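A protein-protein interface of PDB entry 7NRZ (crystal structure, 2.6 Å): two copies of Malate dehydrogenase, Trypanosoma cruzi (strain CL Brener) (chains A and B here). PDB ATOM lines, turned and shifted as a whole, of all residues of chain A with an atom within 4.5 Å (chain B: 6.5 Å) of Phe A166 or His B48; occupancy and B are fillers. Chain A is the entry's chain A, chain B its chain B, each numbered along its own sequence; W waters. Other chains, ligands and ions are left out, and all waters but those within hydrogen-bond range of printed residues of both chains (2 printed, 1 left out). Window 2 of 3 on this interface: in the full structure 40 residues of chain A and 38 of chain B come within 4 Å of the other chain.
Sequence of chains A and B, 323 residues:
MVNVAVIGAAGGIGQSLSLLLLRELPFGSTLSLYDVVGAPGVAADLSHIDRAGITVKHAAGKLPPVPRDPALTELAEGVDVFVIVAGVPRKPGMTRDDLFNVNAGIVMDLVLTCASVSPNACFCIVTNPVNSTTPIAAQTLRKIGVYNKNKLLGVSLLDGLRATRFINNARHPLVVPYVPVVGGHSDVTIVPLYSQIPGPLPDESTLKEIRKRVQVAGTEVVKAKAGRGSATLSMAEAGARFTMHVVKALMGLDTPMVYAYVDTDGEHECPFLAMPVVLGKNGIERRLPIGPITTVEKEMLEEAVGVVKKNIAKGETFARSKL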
ATOM      1  N   LEU A 161      27.591  -6.454  15.365  1.00  0.00           N
ATOM      2  CA  LEU A 161      26.410  -7.257  15.058  1.00  0.00           C
ATOM      3  C   LEU A 161      26.528  -8.636  15.688  1.00  0.00           C
ATOM      4  O   LEU A 161      25.595  -9.128  16.328  1.00  0.00           O
ATOM      5  CB  LEU A 161      26.220  -7.408  13.551  1.00  0.00           C
ATOM      6  CG  LEU A 161      26.343  -6.192  12.634  1.00  0.00           C
ATOM      7  CD1 LEU A 161      25.688  -6.484  11.271  1.00  0.00           C
ATOM      8  CD2 LEU A 161      25.790  -4.900  13.280  1.00  0.00           C
ATOM      9  N   ARG A 162      27.690  -9.244  15.542  1.00  0.00           N
ATOM     10  CA  ARG A 162      27.924 -10.591  16.082  1.00  0.00           C
ATOM     11  C   ARG A 162      27.965 -10.537  17.606  1.00  0.00           C
ATOM     12  O   ARG A 162      27.325 -11.365  18.220  1.00  0.00           O
ATOM     13  CB  ARG A 162      29.200 -11.125  15.448  1.00  0.00           C
ATOM     14  CG  ARG A 162      29.139 -11.301  13.944  1.00  0.00           C
ATOM     15  CD  ARG A 162      30.550 -11.299  13.414  1.00  0.00           C
ATOM     16  NE  ARG A 162      30.633 -11.959  12.128  1.00  0.00           N
ATOM     17  CZ  ARG A 162      31.716 -11.970  11.376  1.00  0.00           C
ATOM     18  NH1 ARG A 162      32.801 -11.343  11.786  1.00  0.00           N
ATOM     19  NH2 ARG A 162      31.707 -12.590  10.215  1.00  0.00           N
ATOM     20  N   ALA A 163      28.620  -9.531  18.174  1.00  0.00           N
ATOM     21  CA  ALA A 163      28.661  -9.413  19.626  1.00  0.00           C
ATOM     22  C   ALA A 163      27.265  -9.202  20.193  1.00  0.00           C
ATOM     23  O   ALA A 163      26.902  -9.798  21.214  1.00  0.00           O
ATOM     24  CB  ALA A 163      29.596  -8.277  20.038  1.00  0.00           C
ATOM     25  N   THR A 164      26.459  -8.372  19.531  1.00  0.00           N
ATOM     26  CA  THR A 164      25.087  -8.172  19.980  1.00  0.00           C
ATOM     27  C   THR A 164      24.262  -9.438  19.802  1.00  0.00           C
ATOM     28  O   THR A 164      23.516  -9.833  20.707  1.00  0.00           O
ATOM     29  CB  THR A 164      24.455  -7.006  19.223  1.00  0.00           C
ATOM     30  OG1 THR A 164      25.259  -5.833  19.398  1.00  0.00           O
ATOM     31  CG2 THR A 164      23.046  -6.742  19.732  1.00  0.00           C
ATOM     32  N   ARG A 165      24.391 -10.095  18.647  1.00  0.00           N
ATOM     33  CA  ARG A 165      23.612 -11.299  18.384  1.00  0.00           C
ATOM     34  C   ARG A 165      23.931 -12.393  19.399  1.00  0.00           C
ATOM     35  O   ARG A 165      23.025 -12.971  20.009  1.00  0.00           O
ATOM     36  CB  ARG A 165      23.871 -11.784  16.955  1.00  0.00           C
ATOM     37  CG  ARG A 165      23.233 -13.114  16.612  1.00  0.00           C
ATOM     38  CD  ARG A 165      21.726 -13.065  16.767  1.00  0.00           C
ATOM     39  NE  ARG A 165      21.038 -13.692  15.644  1.00  0.00           N
ATOM     40  CZ  ARG A 165      19.885 -14.346  15.751  1.00  0.00           C
ATOM     41  NH1 ARG A 165      19.305 -14.466  16.938  1.00  0.00           N
ATOM     42  NH2 ARG A 165      19.317 -14.886  14.678  1.00  0.00           N
ATOM     43  N   PHE A 166      25.222 -12.666  19.616  1.00  0.00           N
ATOM     44  CA  PHE A 166      25.613 -13.790  20.464  1.00  0.00           C
ATOM     45  C   PHE A 166      25.181 -13.578  21.911  1.00  0.00           C
ATOM     46  O   PHE A 166      24.743 -14.526  22.574  1.00  0.00           O
ATOM     47  CB  PHE A 166      27.125 -14.016  20.388  1.00  0.00           C
ATOM     48  CG  PHE A 166      27.627 -14.348  19.006  1.00  0.00           C
ATOM     49  CD1 PHE A 166      26.766 -14.825  18.029  1.00  0.00           C
ATOM     50  CD2 PHE A 166      28.968 -14.172  18.685  1.00  0.00           C
ATOM     51  CE1 PHE A 166      27.229 -15.122  16.759  1.00  0.00           C
ATOM     52  CE2 PHE A 166      29.439 -14.468  17.418  1.00  0.00           C
ATOM     53  CZ  PHE A 166      28.568 -14.943  16.452  1.00  0.00           C
ATOM     54  N   ILE A 167      25.288 -12.349  22.423  1.00  0.00           N
ATOM     55  CA  ILE A 167      24.846 -12.116  23.796  1.00  0.00           C
ATOM     56  C   ILE A 167      23.326 -12.170  23.888  1.00  0.00           C
ATOM     57  O   ILE A 167      22.779 -12.658  24.886  1.00  0.00           O
ATOM     58  CB  ILE A 167      25.410 -10.789  24.347  1.00  0.00           C
ATOM     59  CG1 ILE A 167      25.375 -10.786  25.881  1.00  0.00           C
ATOM     60  CG2 ILE A 167      24.679  -9.577  23.771  1.00  0.00           C
ATOM     61  CD1 ILE A 167      26.342 -11.760  26.516  1.00  0.00           C
ATOM     62  N   ASN A 168      22.616 -11.707  22.854  1.00  0.00           N
ATOM     63  CA  ASN A 168      21.162 -11.818  22.861  1.00  0.00           C
ATOM     64  C   ASN A 168      20.725 -13.275  22.810  1.00  0.00           C
ATOM     65  O   ASN A 168      19.725 -13.648  23.434  1.00  0.00           O
ATOM     66  CB  ASN A 168      20.566 -11.036  21.690  1.00  0.00           C
ATOM     67  CG  ASN A 168      20.602  -9.537  21.909  1.00  0.00           C
ATOM     68  OD1 ASN A 168      20.712  -9.064  23.038  1.00  0.00           O
ATOM     69  ND2 ASN A 168      20.513  -8.781  20.821  1.00  0.00           N
ATOM     70  N   ASN A 169      21.461 -14.114  22.071  1.00  0.00           N
ATOM     71  CA  ASN A 169      21.179 -15.546  22.079  1.00  0.00           C
ATOM     72  C   ASN A 169      21.412 -16.142  23.460  1.00  0.00           C
ATOM     73  O   ASN A 169      20.712 -17.076  23.862  1.00  0.00           O
ATOM     74  CB  ASN A 169      22.044 -16.270  21.048  1.00  0.00           C
ATOM     75  CG  ASN A 169      21.703 -15.888  19.619  1.00  0.00           C
ATOM     76  OD1 ASN A 169      20.650 -15.309  19.347  1.00  0.00           O
ATOM     77  ND2 ASN A 169      22.601 -16.208  18.694  1.00  0.00           N
ATOM     78  N   ALA A 170      22.376 -15.602  24.204  1.00  0.00           N
ATOM     79  CA  ALA A 170      22.731 -16.162  25.502  1.00  0.00           C
ATOM     80  C   ALA A 170      21.709 -15.812  26.578  1.00  0.00           C
ATOM     81  O   ALA A 170      21.391 -16.658  27.423  1.00  0.00           O
ATOM     82  CB  ALA A 170      24.123 -15.684  25.915  1.00  0.00           C
ATOM     83  N   ILE A 210      32.096 -16.522  24.445  1.00  0.00           N
ATOM     84  CA  ILE A 210      31.351 -15.644  23.547  1.00  0.00           C
ATOM     85  C   ILE A 210      32.282 -14.623  22.901  1.00  0.00           C
ATOM     86  O   ILE A 210      32.208 -14.377  21.690  1.00  0.00           O
ATOM     87  CB  ILE A 210      30.190 -14.966  24.299  1.00  0.00           C
ATOM     88  CG1 ILE A 210      29.214 -16.016  24.838  1.00  0.00           C
ATOM     89  CG2 ILE A 210      29.464 -13.994  23.383  1.00  0.00           C
ATOM     90  CD1 ILE A 210      28.032 -15.435  25.585  1.00  0.00           C
ATOM     91  N   ARG A 213      34.301 -16.221  20.260  1.00  0.00           N
ATOM     92  CA  ARG A 213      33.494 -16.465  19.071  1.00  0.00           C
ATOM     93  C   ARG A 213      33.331 -15.197  18.239  1.00  0.00           C
ATOM     94  O   ARG A 213      33.297 -15.263  17.007  1.00  0.00           O
ATOM     95  CB  ARG A 213      32.133 -17.030  19.467  1.00  0.00           C
ATOM     96  CG  ARG A 213      31.416 -17.706  18.320  1.00  0.00           C
ATOM     97  CD  ARG A 213      29.958 -17.945  18.632  1.00  0.00           C
ATOM     98  NE  ARG A 213      29.215 -18.307  17.429  1.00  0.00           N
ATOM     99  CZ  ARG A 213      27.893 -18.420  17.374  1.00  0.00           C
ATOM    100  NH1 ARG A 213      27.303 -18.754  16.234  1.00  0.00           N
ATOM    101  NH2 ARG A 213      27.162 -18.198  18.458  1.00  0.00           N
ATOM    102  N   VAL A 214      33.220 -14.035  18.890  1.00  0.00           N
ATOM    103  CA  VAL A 214      33.208 -12.778  18.146  1.00  0.00           C
ATOM    104  C   VAL A 214      34.520 -12.599  17.394  1.00  0.00           C
ATOM    105  O   VAL A 214      34.538 -12.149  16.242  1.00  0.00           O
ATOM    106  CB  VAL A 214      32.937 -11.588  19.087  1.00  0.00           C
ATOM    107  CG1 VAL A 214      32.969 -10.280  18.303  1.00  0.00           C
ATOM    108  CG2 VAL A 214      31.605 -11.753  19.798  1.00  0.00           C
ATOM    109  N   ALA A 217      34.604 -15.199  14.465  1.00  0.00           N
ATOM    110  CA  ALA A 217      33.345 -15.409  13.756  1.00  0.00           C
ATOM    111  C   ALA A 217      33.534 -15.408  12.243  1.00  0.00           C
ATOM    112  O   ALA A 217      32.794 -16.091  11.527  1.00  0.00           O
ATOM    113  CB  ALA A 217      32.333 -14.339  14.164  1.00  0.00           C
ATOM    114  N   GLU A 220      34.474 -18.789  11.268  1.00  0.00           N
ATOM    115  CA  GLU A 220      33.303 -19.634  11.487  1.00  0.00           C
ATOM    116  C   GLU A 220      32.465 -19.743  10.219  1.00  0.00           C
ATOM    117  O   GLU A 220      31.944 -20.816   9.898  1.00  0.00           O
ATOM    118  CB  GLU A 220      32.469 -19.069  12.639  1.00  0.00           C
ATOM    119  CG  GLU A 220      31.296 -19.937  13.074  1.00  0.00           C
ATOM    120  CD  GLU A 220      30.440 -19.279  14.159  1.00  0.00           C
ATOM    121  OE1 GLU A 220      29.241 -19.034  13.902  1.00  0.00           O
ATOM    122  OE2 GLU A 220      30.955 -19.012  15.269  1.00  0.00           O
ATOM    123  N   VAL A 221      32.329 -18.638   9.483  1.00  0.00           N
ATOM    124  CA  VAL A 221      31.554 -18.650   8.249  1.00  0.00           C
ATOM    125  C   VAL A 221      32.354 -19.280   7.116  1.00  0.00           C
ATOM    126  O   VAL A 221      31.817 -20.065   6.328  1.00  0.00           O
ATOM    127  CB  VAL A 221      31.097 -17.219   7.908  1.00  0.00           C
ATOM    128  CG1 VAL A 221      30.335 -17.196   6.595  1.00  0.00           C
ATOM    129  CG2 VAL A 221      30.234 -16.661   9.028  1.00  0.00           C
ATOM    130  N   SER A 234      25.863 -10.897   5.880  1.00  0.00           N
ATOM    131  CA  SER A 234      25.987 -10.109   7.102  1.00  0.00           C
ATOM    132  C   SER A 234      26.989  -8.973   6.933  1.00  0.00           C
ATOM    133  O   SER A 234      26.852  -7.927   7.579  1.00  0.00           O
ATOM    134  CB  SER A 234      26.380 -11.000   8.283  1.00  0.00           C
ATOM    135  OG  SER A 234      27.653 -11.587   8.097  1.00  0.00           O
ATOM    136  N   LEU B  22      15.257 -12.201   6.521  1.00  0.00           N
ATOM    137  CA  LEU B  22      15.834 -12.092   7.855  1.00  0.00           C
ATOM    138  C   LEU B  22      15.654 -10.687   8.418  1.00  0.00           C
ATOM    139  O   LEU B  22      15.398 -10.516   9.615  1.00  0.00           O
ATOM    140  CB  LEU B  22      17.312 -12.475   7.831  1.00  0.00           C
ATOM    141  CG  LEU B  22      17.961 -12.363   9.210  1.00  0.00           C
ATOM    142  CD1 LEU B  22      17.868 -13.686   9.947  1.00  0.00           C
ATOM    143  CD2 LEU B  22      19.393 -11.907   9.095  1.00  0.00           C
ATOM    144  N   ALA B  43      23.360 -19.948   6.162  1.00  0.00           N
ATOM    145  CA  ALA B  43      22.747 -19.876   7.484  1.00  0.00           C
ATOM    146  C   ALA B  43      23.694 -19.246   8.497  1.00  0.00           C
ATOM    147  O   ALA B  43      23.310 -18.333   9.241  1.00  0.00           O
ATOM    148  CB  ALA B  43      22.321 -21.271   7.938  1.00  0.00           C
ATOM    149  N   ALA B  44      24.942 -19.720   8.536  1.00  0.00           N
ATOM    150  CA  ALA B  44      25.928 -19.143   9.445  1.00  0.00           C
ATOM    151  C   ALA B  44      26.095 -17.649   9.187  1.00  0.00           C
ATOM    152  O   ALA B  44      26.108 -16.842  10.125  1.00  0.00           O
ATOM    153  CB  ALA B  44      27.262 -19.874   9.302  1.00  0.00           C
ATOM    154  N   ASP B  45      26.210 -17.266   7.913  1.00  0.00           N
ATOM    155  CA  ASP B  45      26.313 -15.855   7.548  1.00  0.00           C
ATOM    156  C   ASP B  45      25.142 -15.048   8.104  1.00  0.00           C
ATOM    157  O   ASP B  45      25.336 -14.042   8.798  1.00  0.00           O
ATOM    158  CB  ASP B  45      26.385 -15.732   6.022  1.00  0.00           C
ATOM    159  CG  ASP B  45      26.763 -14.338   5.553  1.00  0.00           C
ATOM    160  OD1 ASP B  45      27.064 -13.468   6.395  1.00  0.00           O
ATOM    161  OD2 ASP B  45      26.754 -14.111   4.327  1.00  0.00           O
ATOM    162  N   LEU B  46      23.912 -15.487   7.820  1.00  0.00           N
ATOM    163  CA  LEU B  46      22.734 -14.735   8.244  1.00  0.00           C
ATOM    164  C   LEU B  46      22.525 -14.795   9.754  1.00  0.00           C
ATOM    165  O   LEU B  46      22.022 -13.831  10.344  1.00  0.00           O
ATOM    166  CB  LEU B  46      21.497 -15.254   7.513  1.00  0.00           C
ATOM    167  CG  LEU B  46      21.401 -14.895   6.028  1.00  0.00           C
ATOM    168  CD1 LEU B  46      20.281 -15.673   5.352  1.00  0.00           C
ATOM    169  CD2 LEU B  46      21.202 -13.391   5.852  1.00  0.00           C
ATOM    170  N   SER B  47      22.907 -15.903  10.397  1.00  0.00           N
ATOM    171  CA  SER B  47      22.716 -16.025  11.837  1.00  0.00           C
ATOM    172  C   SER B  47      23.506 -14.985  12.619  1.00  0.00           C
ATOM    173  O   SER B  47      23.165 -14.704  13.774  1.00  0.00           O
ATOM    174  CB  SER B  47      23.116 -17.423  12.307  1.00  0.00           C
ATOM    175  OG  SER B  47      24.515 -17.615  12.199  1.00  0.00           O
ATOM    176  N   HIS B  48      24.555 -14.414  12.022  1.00  0.00           N
ATOM    177  CA  HIS B  48      25.388 -13.436  12.708  1.00  0.00           C
ATOM    178  C   HIS B  48      24.768 -12.046  12.754  1.00  0.00           C
ATOM    179  O   HIS B  48      25.268 -11.193  13.494  1.00  0.00           O
ATOM    180  CB  HIS B  48      26.762 -13.359  12.043  1.00  0.00           C
ATOM    181  CG  HIS B  48      27.642 -14.527  12.353  1.00  0.00           C
ATOM    182  ND1 HIS B  48      28.989 -14.542  12.067  1.00  0.00           N
ATOM    183  CD2 HIS B  48      27.365 -15.722  12.927  1.00  0.00           C
ATOM    184  CE1 HIS B  48      29.506 -15.697  12.451  1.00  0.00           C
ATOM    185  NE2 HIS B  48      28.540 -16.429  12.976  1.00  0.00           N
ATOM    186  N   ILE B  49      23.703 -11.795  11.989  1.00  0.00           N
ATOM    187  CA  ILE B  49      23.059 -10.489  12.017  1.00  0.00           C
ATOM    188  C   ILE B  49      22.264 -10.344  13.307  1.00  0.00           C
ATOM    189  O   ILE B  49      21.669 -11.310  13.805  1.00  0.00           O
ATOM    190  CB  ILE B  49      22.175 -10.305  10.771  1.00  0.00           C
ATOM    191  CG1 ILE B  49      23.053 -10.278   9.516  1.00  0.00           C
ATOM    192  CG2 ILE B  49      21.335  -9.040  10.877  1.00  0.00           C
ATOM    193  CD1 ILE B  49      22.297 -10.088   8.218  1.00  0.00           C
ATOM    194  N   ASP B  50      22.255  -9.129  13.860  1.00  0.00           N
ATOM    195  CA  ASP B  50      21.679  -8.886  15.176  1.00  0.00           C
ATOM    196  C   ASP B  50      20.162  -8.749  15.133  1.00  0.00           C
ATOM    197  O   ASP B  50      19.601  -7.779  15.657  1.00  0.00           O
ATOM    198  CB  ASP B  50      22.311  -7.642  15.811  1.00  0.00           C
ATOM    199  CG  ASP B  50      22.224  -6.415  14.920  1.00  0.00           C
ATOM    200  OD1 ASP B  50      21.852  -6.541  13.733  1.00  0.00           O
ATOM    201  OD2 ASP B  50      22.536  -5.310  15.410  1.00  0.00           O
ATOM    202  N   ARG B  51      19.486  -9.712  14.509  1.00  0.00           N
ATOM    203  CA  ARG B  51      18.049  -9.846  14.700  1.00  0.00           C
ATOM    204  C   ARG B  51      17.788 -10.475  16.061  1.00  0.00           C
ATOM    205  O   ARG B  51      18.408 -11.482  16.418  1.00  0.00           O
ATOM    206  CB  ARG B  51      17.424 -10.706  13.599  1.00  0.00           C
ATOM    207  CG  ARG B  51      17.067  -9.976  12.306  1.00  0.00           C
ATOM    208  CD  ARG B  51      16.309  -8.661  12.534  1.00  0.00           C
ATOM    209  NE  ARG B  51      15.092  -8.804  13.334  1.00  0.00           N
ATOM    210  CZ  ARG B  51      13.901  -9.163  12.853  1.00  0.00           C
ATOM    211  NH1 ARG B  51      12.854  -9.250  13.664  1.00  0.00           N
ATOM    212  NH2 ARG B  51      13.751  -9.439  11.565  1.00  0.00           N
HETATM  213  O   HOH W   1      28.974 -13.364   9.398  1.00  0.00           O
HETATM  214  O   HOH W   2      24.063  -3.862  17.115  1.00  0.00           O
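Phe A166 touches one residue of chain B. Of chain A, only Leu A161, Arg A162, Arg A165, Phe A166, Ala A217, Glu A220 and Val A221 come within 4 Å of His B48. Of the printed residues of chain B, Leu A161 touches His B48 and Asp B50. Of the printed residues of chain A, Ile B49 touches Arg A165 (3.1 Å) and Ser A234 (3.6 Å). Of the printed residues of chain A, Asp B45 touches Ser A234. Of the printed residues of chain A, Asp B50 touches Leu A161. Of the printed residues of chain B, Ala A217 touches His B48 (3.4 Å). The nearest residue of chain B that does not touch Phe A166 is Ser B47 (5.1 Å).
Of the 17 printed residues of chain A, 8 touch a printed residue of chain B. Printed residues of chain A that touch a printed residue of chain B: Leu A161, Arg A162, Arg A165, Phe A166, Ala A217, Glu A220, Val A221 and Ser A234. Hydrophobic or aromatic side chains of chain A within 4 Å of the printed part of chain B: Leu A161, Phe A166, Ala A217 and Val A221. Among the printed residues, no Asp or Glu carboxylate lies within 4 Å of a Lys or Arg side-chain nitrogen of the other chain.
The side-chain hydroxyl (OG) of Ser B47 sits close to the backbone carbonyl oxygen (O) of Ala B43, 3.3 Å away. The backbone carbonyl oxygen (O) of Ala B44 is in hydrogen-bond range of the side-chain hydroxyl (OG) of Ser B47, 2.7 Å away. The backbone carbonyl oxygen (O) of Leu B22 is in hydrogen-bond range of the guanidinium group (NH2) of Arg B51 (2.8 Å). The side-chain carboxylate (OE2) of Glu A220 is in salt-bridge range of the guanidinium group (NE) of Arg A213, 2.9 Å away. The side-chain amide oxygen (OD1) of Asn A169 is in hydrogen-bond range of the guanidinium group (NH1) of Arg A165 (2.9 Å).
No position is printed for both chains. Of the 13 pairs that touch across the chains among the printed residues, none has its exchanged pair printed and touching as well.
Leu A161 touches His B48. CB of Asp B50 touches O of Leu A161, 3.6 Å away. O of His B48 touches CB of Arg A165, 3.8 Å away. Phe A166 touches His B48 (CZ to NE2, 3.8 Å). O of Ala A217 touches CE1 of His B48 (3.4 Å). CE1 of His B48 touches CG2 of Val A221 (3.6 Å). Ser A234 touches Ile B49.
Water W1 lies within hydrogen-bond range of the side-chain hydroxyl of Ser A234 (2.6 Å), a ring nitrogen (ND1) of His B48 (2.9 Å) and the guanidinium group of Arg A162 (3.0 Å). Water W2 bridges the side-chain carboxylate (OD2) of Asp B50 (2.7 Å) and the side-chain hydroxyl (OG1) of Thr A164 (3.2 Å).
The guanidinium group (NE) of Arg A165 lies within hydrogen-bond range of the backbone carbonyl oxygen (O) of Ile B49 (3.1 Å). The guanidinium group (NH1) of Arg A165 is in hydrogen-bond range of the backbone carbonyl oxygen (O) of Arg B51 (3.2 Å). The side-chain carboxylate (OE1) of Glu A220 is in hydrogen-bond range of a ring nitrogen (NE2) of His B48 (2.9 Å). OD1 of Asp B45 sits at hydrogen-bond distance from OG of Ser A234, 2.6 Å away. NE of Arg A162 sits at hydrogen-bond distance from ND1 of His B48. The guanidinium group (NE) of Arg A165 is in hydrogen-bond range of the backbone carbonyl oxygen (O) of Ser B47 (3.0 Å).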
